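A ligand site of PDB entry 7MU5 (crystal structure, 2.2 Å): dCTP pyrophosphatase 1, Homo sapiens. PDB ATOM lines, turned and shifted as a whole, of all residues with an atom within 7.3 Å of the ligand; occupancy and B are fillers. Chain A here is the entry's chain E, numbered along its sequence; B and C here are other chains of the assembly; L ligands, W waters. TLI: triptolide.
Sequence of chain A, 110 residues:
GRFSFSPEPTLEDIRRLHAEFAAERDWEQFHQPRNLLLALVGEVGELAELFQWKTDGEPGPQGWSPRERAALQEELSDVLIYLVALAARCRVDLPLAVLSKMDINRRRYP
NE2 of His 31 is in hydrogen-bond range of O25 of the ligand (3.2 Å). OH of Tyr 82 sits at hydrogen-bond distance from O25 of the ligand, at 3.4 Å.
The side-chain amide nitrogen of Asn 35 is in hydrogen-bond range of the backbone carbonyl oxygen of Phe 30 (2.8 Å). N of Trp 27 sits at hydrogen-bond distance from O of Ala 22 (3.1 Å). The indole nitrogen (NE1) of Trp 53 of chain B sits close to the side-chain amide nitrogen (NE2) of Gln 52 of chain B (3.1 Å).
Residues that only touch the ligand: Trp 27 (3.2 Å), Trp 53 of chain B (3.3 Å), Phe 30 (3.7 Å) and Tyr 109 of chain C (3.99 Å). Of the 20 residues printed, 6 come within 4 Å of the ligand.
Water W1 lies within hydrogen-bond range of NE2 of His 18 (2.8 Å) and O25 of the ligand (2.8 Å).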
ATOM      1  N   HIS A  18       1.808   3.488 -16.402  1.00  0.00           N
ATOM      2  CA  HIS A  18       1.846   4.926 -16.587  1.00  0.00           C
ATOM      3  C   HIS A  18       3.220   5.396 -17.049  1.00  0.00           C
ATOM      4  O   HIS A  18       3.308   6.328 -17.853  1.00  0.00           O
ATOM      5  CB  HIS A  18       1.476   5.684 -15.314  1.00  0.00           C
ATOM      6  CG  HIS A  18       1.576   7.165 -15.506  1.00  0.00           C
ATOM      7  ND1 HIS A  18       2.721   7.870 -15.227  1.00  0.00           N
ATOM      8  CD2 HIS A  18       0.699   8.053 -16.031  1.00  0.00           C
ATOM      9  CE1 HIS A  18       2.539   9.152 -15.558  1.00  0.00           C
ATOM     10  NE2 HIS A  18       1.323   9.281 -16.028  1.00  0.00           N
ATOM     11  N   PHE A  21       3.237   4.517 -20.799  1.00  0.00           N
ATOM     12  CA  PHE A  21       2.403   5.549 -21.428  1.00  0.00           C
ATOM     13  C   PHE A  21       3.164   6.854 -21.574  1.00  0.00           C
ATOM     14  O   PHE A  21       3.268   7.411 -22.667  1.00  0.00           O
ATOM     15  CB  PHE A  21       1.133   5.731 -20.602  1.00  0.00           C
ATOM     16  CG  PHE A  21       0.260   6.870 -21.064  1.00  0.00           C
ATOM     17  CD1 PHE A  21      -0.685   6.672 -22.047  1.00  0.00           C
ATOM     18  CD2 PHE A  21       0.408   8.140 -20.531  1.00  0.00           C
ATOM     19  CE1 PHE A  21      -1.441   7.690 -22.481  1.00  0.00           C
ATOM     20  CE2 PHE A  21      -0.383   9.178 -20.973  1.00  0.00           C
ATOM     21  CZ  PHE A  21      -1.288   8.955 -21.956  1.00  0.00           C
ATOM     22  N   ALA A  22       3.756   7.342 -20.487  1.00  0.00           N
ATOM     23  CA  ALA A  22       4.474   8.610 -20.509  1.00  0.00           C
ATOM     24  C   ALA A  22       5.755   8.549 -21.341  1.00  0.00           C
ATOM     25  O   ALA A  22       6.114   9.527 -22.010  1.00  0.00           O
ATOM     26  CB  ALA A  22       4.787   9.022 -19.078  1.00  0.00           C
ATOM     27  N   ARG A  25       5.372   8.828 -25.129  1.00  0.00           N
ATOM     28  CA  ARG A  25       4.924  10.126 -25.652  1.00  0.00           C
ATOM     29  C   ARG A  25       5.935  11.231 -25.394  1.00  0.00           C
ATOM     30  O   ARG A  25       5.654  12.379 -25.731  1.00  0.00           O
ATOM     31  CB  ARG A  25       3.557  10.499 -25.040  1.00  0.00           C
ATOM     32  CG  ARG A  25       2.397   9.778 -25.681  1.00  0.00           C
ATOM     33  CD  ARG A  25       1.211   9.594 -24.781  1.00  0.00           C
ATOM     34  NE  ARG A  25       0.252   8.670 -25.384  1.00  0.00           N
ATOM     35  CZ  ARG A  25       0.369   7.343 -25.395  1.00  0.00           C
ATOM     36  NH1 ARG A  25       1.398   6.747 -24.807  1.00  0.00           N
ATOM     37  NH2 ARG A  25      -0.553   6.599 -26.006  1.00  0.00           N
ATOM     38  N   ASP A  26       7.115  10.901 -24.809  1.00  0.00           N
ATOM     39  CA  ASP A  26       8.140  11.876 -24.389  1.00  0.00           C
ATOM     40  C   ASP A  26       7.567  12.932 -23.434  1.00  0.00           C
ATOM     41  O   ASP A  26       7.798  14.134 -23.568  1.00  0.00           O
ATOM     42  CB  ASP A  26       8.812  12.532 -25.598  1.00  0.00           C
ATOM     43  CG  ASP A  26      10.052  13.365 -25.218  1.00  0.00           C
ATOM     44  OD1 ASP A  26      10.955  12.839 -24.503  1.00  0.00           O
ATOM     45  OD2 ASP A  26      10.113  14.537 -25.627  1.00  0.00           O
ATOM     46  N   TRP A  27       6.842  12.462 -22.417  1.00  0.00           N
ATOM     47  CA  TRP A  27       6.268  13.329 -21.398  1.00  0.00           C
ATOM     48  C   TRP A  27       7.071  13.335 -20.110  1.00  0.00           C
ATOM     49  O   TRP A  27       6.833  14.210 -19.264  1.00  0.00           O
ATOM     50  CB  TRP A  27       4.833  12.906 -21.098  1.00  0.00           C
ATOM     51  CG  TRP A  27       3.860  13.215 -22.183  1.00  0.00           C
ATOM     52  CD1 TRP A  27       4.104  13.814 -23.403  1.00  0.00           C
ATOM     53  CD2 TRP A  27       2.471  12.942 -22.149  1.00  0.00           C
ATOM     54  NE1 TRP A  27       2.932  13.909 -24.119  1.00  0.00           N
ATOM     55  CE2 TRP A  27       1.913  13.385 -23.369  1.00  0.00           C
ATOM     56  CE3 TRP A  27       1.623  12.344 -21.186  1.00  0.00           C
ATOM     57  CZ2 TRP A  27       0.565  13.273 -23.650  1.00  0.00           C
ATOM     58  CZ3 TRP A  27       0.294  12.229 -21.480  1.00  0.00           C
ATOM     59  CH2 TRP A  27      -0.226  12.689 -22.696  1.00  0.00           C
ATOM     60  N   GLU A  28       8.021  12.397 -19.962  1.00  0.00           N
ATOM     61  CA  GLU A  28       8.759  12.312 -18.709  1.00  0.00           C
ATOM     62  C   GLU A  28       9.526  13.592 -18.423  1.00  0.00           C
ATOM     63  O   GLU A  28       9.703  13.970 -17.254  1.00  0.00           O
ATOM     64  CB  GLU A  28       9.701  11.099 -18.748  1.00  0.00           C
ATOM     65  CG  GLU A  28       8.969   9.800 -18.411  1.00  0.00           C
ATOM     66  CD  GLU A  28       9.916   8.712 -17.900  1.00  0.00           C
ATOM     67  OE1 GLU A  28      10.996   9.054 -17.330  1.00  0.00           O
ATOM     68  OE2 GLU A  28       9.577   7.509 -18.067  1.00  0.00           O
ATOM     69  N   PHE A  30       8.390  16.449 -18.524  1.00  0.00           N
ATOM     70  CA  PHE A  30       7.490  17.368 -17.839  1.00  0.00           C
ATOM     71  C   PHE A  30       7.095  16.895 -16.445  1.00  0.00           C
ATOM     72  O   PHE A  30       6.293  17.559 -15.791  1.00  0.00           O
ATOM     73  CB  PHE A  30       6.200  17.556 -18.635  1.00  0.00           C
ATOM     74  CG  PHE A  30       6.437  17.878 -20.080  1.00  0.00           C
ATOM     75  CD1 PHE A  30       6.918  19.124 -20.454  1.00  0.00           C
ATOM     76  CD2 PHE A  30       6.182  16.935 -21.055  1.00  0.00           C
ATOM     77  CE1 PHE A  30       7.136  19.420 -21.791  1.00  0.00           C
ATOM     78  CE2 PHE A  30       6.386  17.229 -22.388  1.00  0.00           C
ATOM     79  CZ  PHE A  30       6.868  18.475 -22.761  1.00  0.00           C
ATOM     80  N   HIS A  31       7.621  15.761 -15.986  1.00  0.00           N
ATOM     81  CA  HIS A  31       7.164  15.128 -14.761  1.00  0.00           C
ATOM     82  C   HIS A  31       8.106  15.345 -13.589  1.00  0.00           C
ATOM     83  O   HIS A  31       8.300  14.470 -12.741  1.00  0.00           O
ATOM     84  CB  HIS A  31       6.909  13.650 -15.025  1.00  0.00           C
ATOM     85  CG  HIS A  31       5.746  13.417 -15.953  1.00  0.00           C
ATOM     86  ND1 HIS A  31       5.383  12.173 -16.408  1.00  0.00           N
ATOM     87  CD2 HIS A  31       4.857  14.291 -16.491  1.00  0.00           C
ATOM     88  CE1 HIS A  31       4.324  12.286 -17.202  1.00  0.00           C
ATOM     89  NE2 HIS A  31       3.973  13.564 -17.246  1.00  0.00           N
ATOM     90  N   ASN A  35       5.621  19.588 -10.701  1.00  0.00           N
ATOM     91  CA  ASN A  35       4.608  19.541 -11.763  1.00  0.00           C
ATOM     92  C   ASN A  35       3.547  18.492 -11.431  1.00  0.00           C
ATOM     93  O   ASN A  35       2.336  18.746 -11.567  1.00  0.00           O
ATOM     94  CB  ASN A  35       5.243  19.230 -13.129  1.00  0.00           C
ATOM     95  CG  ASN A  35       5.998  20.425 -13.739  1.00  0.00           C
ATOM     96  OD1 ASN A  35       6.242  21.428 -13.099  1.00  0.00           O
ATOM     97  ND2 ASN A  35       6.410  20.265 -14.983  1.00  0.00           N
ATOM     98  N   LEU A  36       3.994  17.304 -11.037  1.00  0.00           N
ATOM     99  CA  LEU A  36       3.082  16.213 -10.740  1.00  0.00           C
ATOM    100  C   LEU A  36       2.257  16.524  -9.505  1.00  0.00           C
ATOM    101  O   LEU A  36       1.073  16.162  -9.440  1.00  0.00           O
ATOM    102  CB  LEU A  36       3.836  14.897 -10.543  1.00  0.00           C
ATOM    103  CG  LEU A  36       4.689  14.376 -11.722  1.00  0.00           C
ATOM    104  CD1 LEU A  36       5.580  13.187 -11.328  1.00  0.00           C
ATOM    105  CD2 LEU A  36       3.849  13.969 -12.878  1.00  0.00           C
ATOM    106  N   ALA A  39      -0.457  18.763 -10.660  1.00  0.00           N
ATOM    107  CA  ALA A  39      -1.428  18.016 -11.450  1.00  0.00           C
ATOM    108  C   ALA A  39      -2.321  17.205 -10.534  1.00  0.00           C
ATOM    109  O   ALA A  39      -3.529  17.061 -10.768  1.00  0.00           O
ATOM    110  CB  ALA A  39      -0.733  17.109 -12.458  1.00  0.00           C
ATOM    111  N   TYR A  82      -1.702  10.156 -10.772  1.00  0.00           N
ATOM    112  CA  TYR A  82      -0.716  11.207 -10.488  1.00  0.00           C
ATOM    113  C   TYR A  82      -0.023  10.995  -9.156  1.00  0.00           C
ATOM    114  O   TYR A  82       1.149  11.339  -9.006  1.00  0.00           O
ATOM    115  CB  TYR A  82      -1.397  12.579 -10.532  1.00  0.00           C
ATOM    116  CG  TYR A  82      -1.542  13.159 -11.917  1.00  0.00           C
ATOM    117  CD1 TYR A  82      -0.461  13.198 -12.782  1.00  0.00           C
ATOM    118  CD2 TYR A  82      -2.756  13.664 -12.368  1.00  0.00           C
ATOM    119  CE1 TYR A  82      -0.566  13.713 -14.050  1.00  0.00           C
ATOM    120  CE2 TYR A  82      -2.870  14.185 -13.659  1.00  0.00           C
ATOM    121  CZ  TYR A  82      -1.762  14.188 -14.499  1.00  0.00           C
ATOM    122  OH  TYR A  82      -1.814  14.689 -15.790  1.00  0.00           O
ATOM    123  N   GLU B  49      -4.101  23.833 -12.254  1.00  0.00           N
ATOM    124  CA  GLU B  49      -4.059  23.248 -13.611  1.00  0.00           C
ATOM    125  C   GLU B  49      -3.390  24.239 -14.569  1.00  0.00           C
ATOM    126  O   GLU B  49      -2.656  23.785 -15.412  1.00  0.00           O
ATOM    127  CB  GLU B  49      -5.451  22.788 -14.023  1.00  0.00           C
ATOM    128  CG  GLU B  49      -5.482  21.909 -15.267  1.00  0.00           C
ATOM    129  CD  GLU B  49      -5.736  22.620 -16.573  1.00  0.00           C
ATOM    130  OE1 GLU B  49      -6.681  23.404 -16.633  1.00  0.00           O
ATOM    131  OE2 GLU B  49      -5.015  22.352 -17.543  1.00  0.00           O
ATOM    132  N   GLN B  52       0.554  23.795 -13.641  1.00  0.00           N
ATOM    133  CA  GLN B  52       1.145  22.440 -13.468  1.00  0.00           C
ATOM    134  C   GLN B  52       2.312  22.092 -14.407  1.00  0.00           C
ATOM    135  O   GLN B  52       3.169  21.437 -13.931  1.00  0.00           O
ATOM    136  CB  GLN B  52       0.053  21.358 -13.528  1.00  0.00           C
ATOM    137  CG  GLN B  52      -0.520  21.100 -14.917  1.00  0.00           C
ATOM    138  CD  GLN B  52      -1.848  20.385 -14.929  1.00  0.00           C
ATOM    139  OE1 GLN B  52      -2.452  20.150 -13.906  1.00  0.00           O
ATOM    140  NE2 GLN B  52      -2.321  20.058 -16.117  1.00  0.00           N
ATOM    141  N   TRP B  53       2.303  22.476 -15.682  1.00  0.00           N
ATOM    142  CA  TRP B  53       3.362  22.157 -16.684  1.00  0.00           C
ATOM    143  C   TRP B  53       4.193  23.405 -16.964  1.00  0.00           C
ATOM    144  O   TRP B  53       5.021  23.338 -17.865  1.00  0.00           O
ATOM    145  CB  TRP B  53       2.756  21.563 -17.962  1.00  0.00           C
ATOM    146  CG  TRP B  53       1.772  20.456 -17.787  1.00  0.00           C
ATOM    147  CD1 TRP B  53       0.550  20.374 -18.385  1.00  0.00           C
ATOM    148  CD2 TRP B  53       1.934  19.237 -17.038  1.00  0.00           C
ATOM    149  NE1 TRP B  53      -0.081  19.217 -18.031  1.00  0.00           N
ATOM    150  CE2 TRP B  53       0.739  18.494 -17.210  1.00  0.00           C
ATOM    151  CE3 TRP B  53       2.932  18.704 -16.225  1.00  0.00           C
ATOM    152  CZ2 TRP B  53       0.529  17.273 -16.596  1.00  0.00           C
ATOM    153  CZ3 TRP B  53       2.729  17.482 -15.632  1.00  0.00           C
ATOM    154  CH2 TRP B  53       1.543  16.772 -15.817  1.00  0.00           C
ATOM    155  N   LYS B  54       4.015  24.475 -16.185  1.00  0.00           N
ATOM    156  CA  LYS B  54       4.712  25.777 -16.387  1.00  0.00           C
ATOM    157  C   LYS B  54       5.736  25.981 -15.284  1.00  0.00           C
ATOM    158  O   LYS B  54       5.407  26.631 -14.296  1.00  0.00           O
ATOM    159  CB  LYS B  54       3.707  26.933 -16.455  1.00  0.00           C
ATOM    160  CG  LYS B  54       2.781  26.904 -17.666  1.00  0.00           C
ATOM    161  CD  LYS B  54       1.905  28.114 -17.742  1.00  0.00           C
ATOM    162  CE  LYS B  54       1.233  28.332 -19.075  1.00  0.00           C
ATOM    163  NZ  LYS B  54       2.041  29.163 -19.995  1.00  0.00           N
ATOM    164  N   GLU B  68      -4.566  32.526 -21.538  1.00  0.00           N
ATOM    165  CA  GLU B  68      -3.948  31.991 -20.293  1.00  0.00           C
ATOM    166  C   GLU B  68      -4.083  33.033 -19.187  1.00  0.00           C
ATOM    167  O   GLU B  68      -4.399  32.648 -18.082  1.00  0.00           O
ATOM    168  CB  GLU B  68      -2.482  31.601 -20.507  1.00  0.00           C
ATOM    169  CG  GLU B  68      -2.246  30.244 -21.139  1.00  0.00           C
ATOM    170  CD  GLU B  68      -0.835  30.009 -21.664  1.00  0.00           C
ATOM    171  OE1 GLU B  68      -0.010  30.933 -21.648  1.00  0.00           O
ATOM    172  OE2 GLU B  68      -0.560  28.893 -22.097  1.00  0.00           O
ATOM    173  N   ASN C 105      -7.168   7.413 -21.634  1.00  0.00           N
ATOM    174  CA  ASN C 105      -5.979   8.234 -21.843  1.00  0.00           C
ATOM    175  C   ASN C 105      -5.314   7.896 -23.174  1.00  0.00           C
ATOM    176  O   ASN C 105      -4.796   8.785 -23.858  1.00  0.00           O
ATOM    177  CB  ASN C 105      -4.956   8.073 -20.712  1.00  0.00           C
ATOM    178  CG  ASN C 105      -5.337   8.817 -19.451  1.00  0.00           C
ATOM    179  OD1 ASN C 105      -6.264   9.613 -19.439  1.00  0.00           O
ATOM    180  ND2 ASN C 105      -4.607   8.541 -18.366  1.00  0.00           N
ATOM    181  N   TYR C 109      -4.838  10.312 -26.514  1.00  0.00           N
ATOM    182  CA  TYR C 109      -3.519  10.585 -27.064  1.00  0.00           C
ATOM    183  C   TYR C 109      -2.969   9.393 -27.879  1.00  0.00           C
ATOM    184  O   TYR C 109      -3.312   9.232 -29.069  1.00  0.00           O
ATOM    185  CB  TYR C 109      -2.549  10.937 -25.935  1.00  0.00           C
ATOM    186  CG  TYR C 109      -3.030  12.082 -25.059  1.00  0.00           C
ATOM    187  CD1 TYR C 109      -2.771  13.415 -25.407  1.00  0.00           C
ATOM    188  CD2 TYR C 109      -3.736  11.829 -23.882  1.00  0.00           C
ATOM    189  CE1 TYR C 109      -3.201  14.458 -24.599  1.00  0.00           C
ATOM    190  CE2 TYR C 109      -4.152  12.861 -23.059  1.00  0.00           C
ATOM    191  CZ  TYR C 109      -3.886  14.176 -23.433  1.00  0.00           C
ATOM    192  OH  TYR C 109      -4.324  15.197 -22.632  1.00  0.00           O
HETATM  193  C01 TLI L   1       2.429  23.843 -24.094  1.00  0.00           C
HETATM  194  C02 TLI L   1       0.932  23.525 -23.950  1.00  0.00           C
HETATM  195  C03 TLI L   1       0.078  23.817 -25.210  1.00  0.00           C
HETATM  196  C04 TLI L   1       0.870  22.064 -23.435  1.00  0.00           C
HETATM  197  C05 TLI L   1       1.393  21.707 -22.059  1.00  0.00           C
HETATM  198  C07 TLI L   1       2.145  20.453 -21.751  1.00  0.00           C
HETATM  199  C08 TLI L   1       1.605  19.164 -22.397  1.00  0.00           C
HETATM  200  C10 TLI L   1       1.544  17.993 -21.373  1.00  0.00           C
HETATM  201  C11 TLI L   1       2.624  17.577 -20.369  1.00  0.00           C
HETATM  202  C12 TLI L   1       2.489  16.152 -19.777  1.00  0.00           C
HETATM  203  C13 TLI L   1       1.085  15.632 -19.710  1.00  0.00           C
HETATM  204  C14 TLI L   1       0.091  15.963 -20.594  1.00  0.00           C
HETATM  205  C15 TLI L   1       0.151  17.284 -21.315  1.00  0.00           C
HETATM  206  C16 TLI L   1      -0.668  17.248 -22.649  1.00  0.00           C
HETATM  207  C17 TLI L   1      -0.681  18.585 -23.401  1.00  0.00           C
HETATM  208  C18 TLI L   1       0.464  19.576 -23.361  1.00  0.00           C
HETATM  209  C19 TLI L   1       0.418  20.860 -24.281  1.00  0.00           C
HETATM  210  C22 TLI L   1      -1.164  15.186 -20.201  1.00  0.00           C
HETATM  211  C24 TLI L   1       0.498  14.656 -18.771  1.00  0.00           C
HETATM  212  C26 TLI L   1       2.295  17.000 -22.495  1.00  0.00           C
HETATM  213  O06 TLI L   1       0.023  21.862 -22.263  1.00  0.00           O
HETATM  214  O09 TLI L   1       2.905  19.679 -22.654  1.00  0.00           O
HETATM  215  O20 TLI L   1       1.320  20.694 -25.289  1.00  0.00           O
HETATM  216  O21 TLI L   1       0.270  18.691 -24.407  1.00  0.00           O
HETATM  217  O23 TLI L   1      -0.749  14.288 -19.201  1.00  0.00           O
HETATM  218  O25 TLI L   1       0.915  14.178 -17.763  1.00  0.00           O
HETATM  219  O   HOH W   1       0.242  11.449 -17.473  1.00  0.00           O
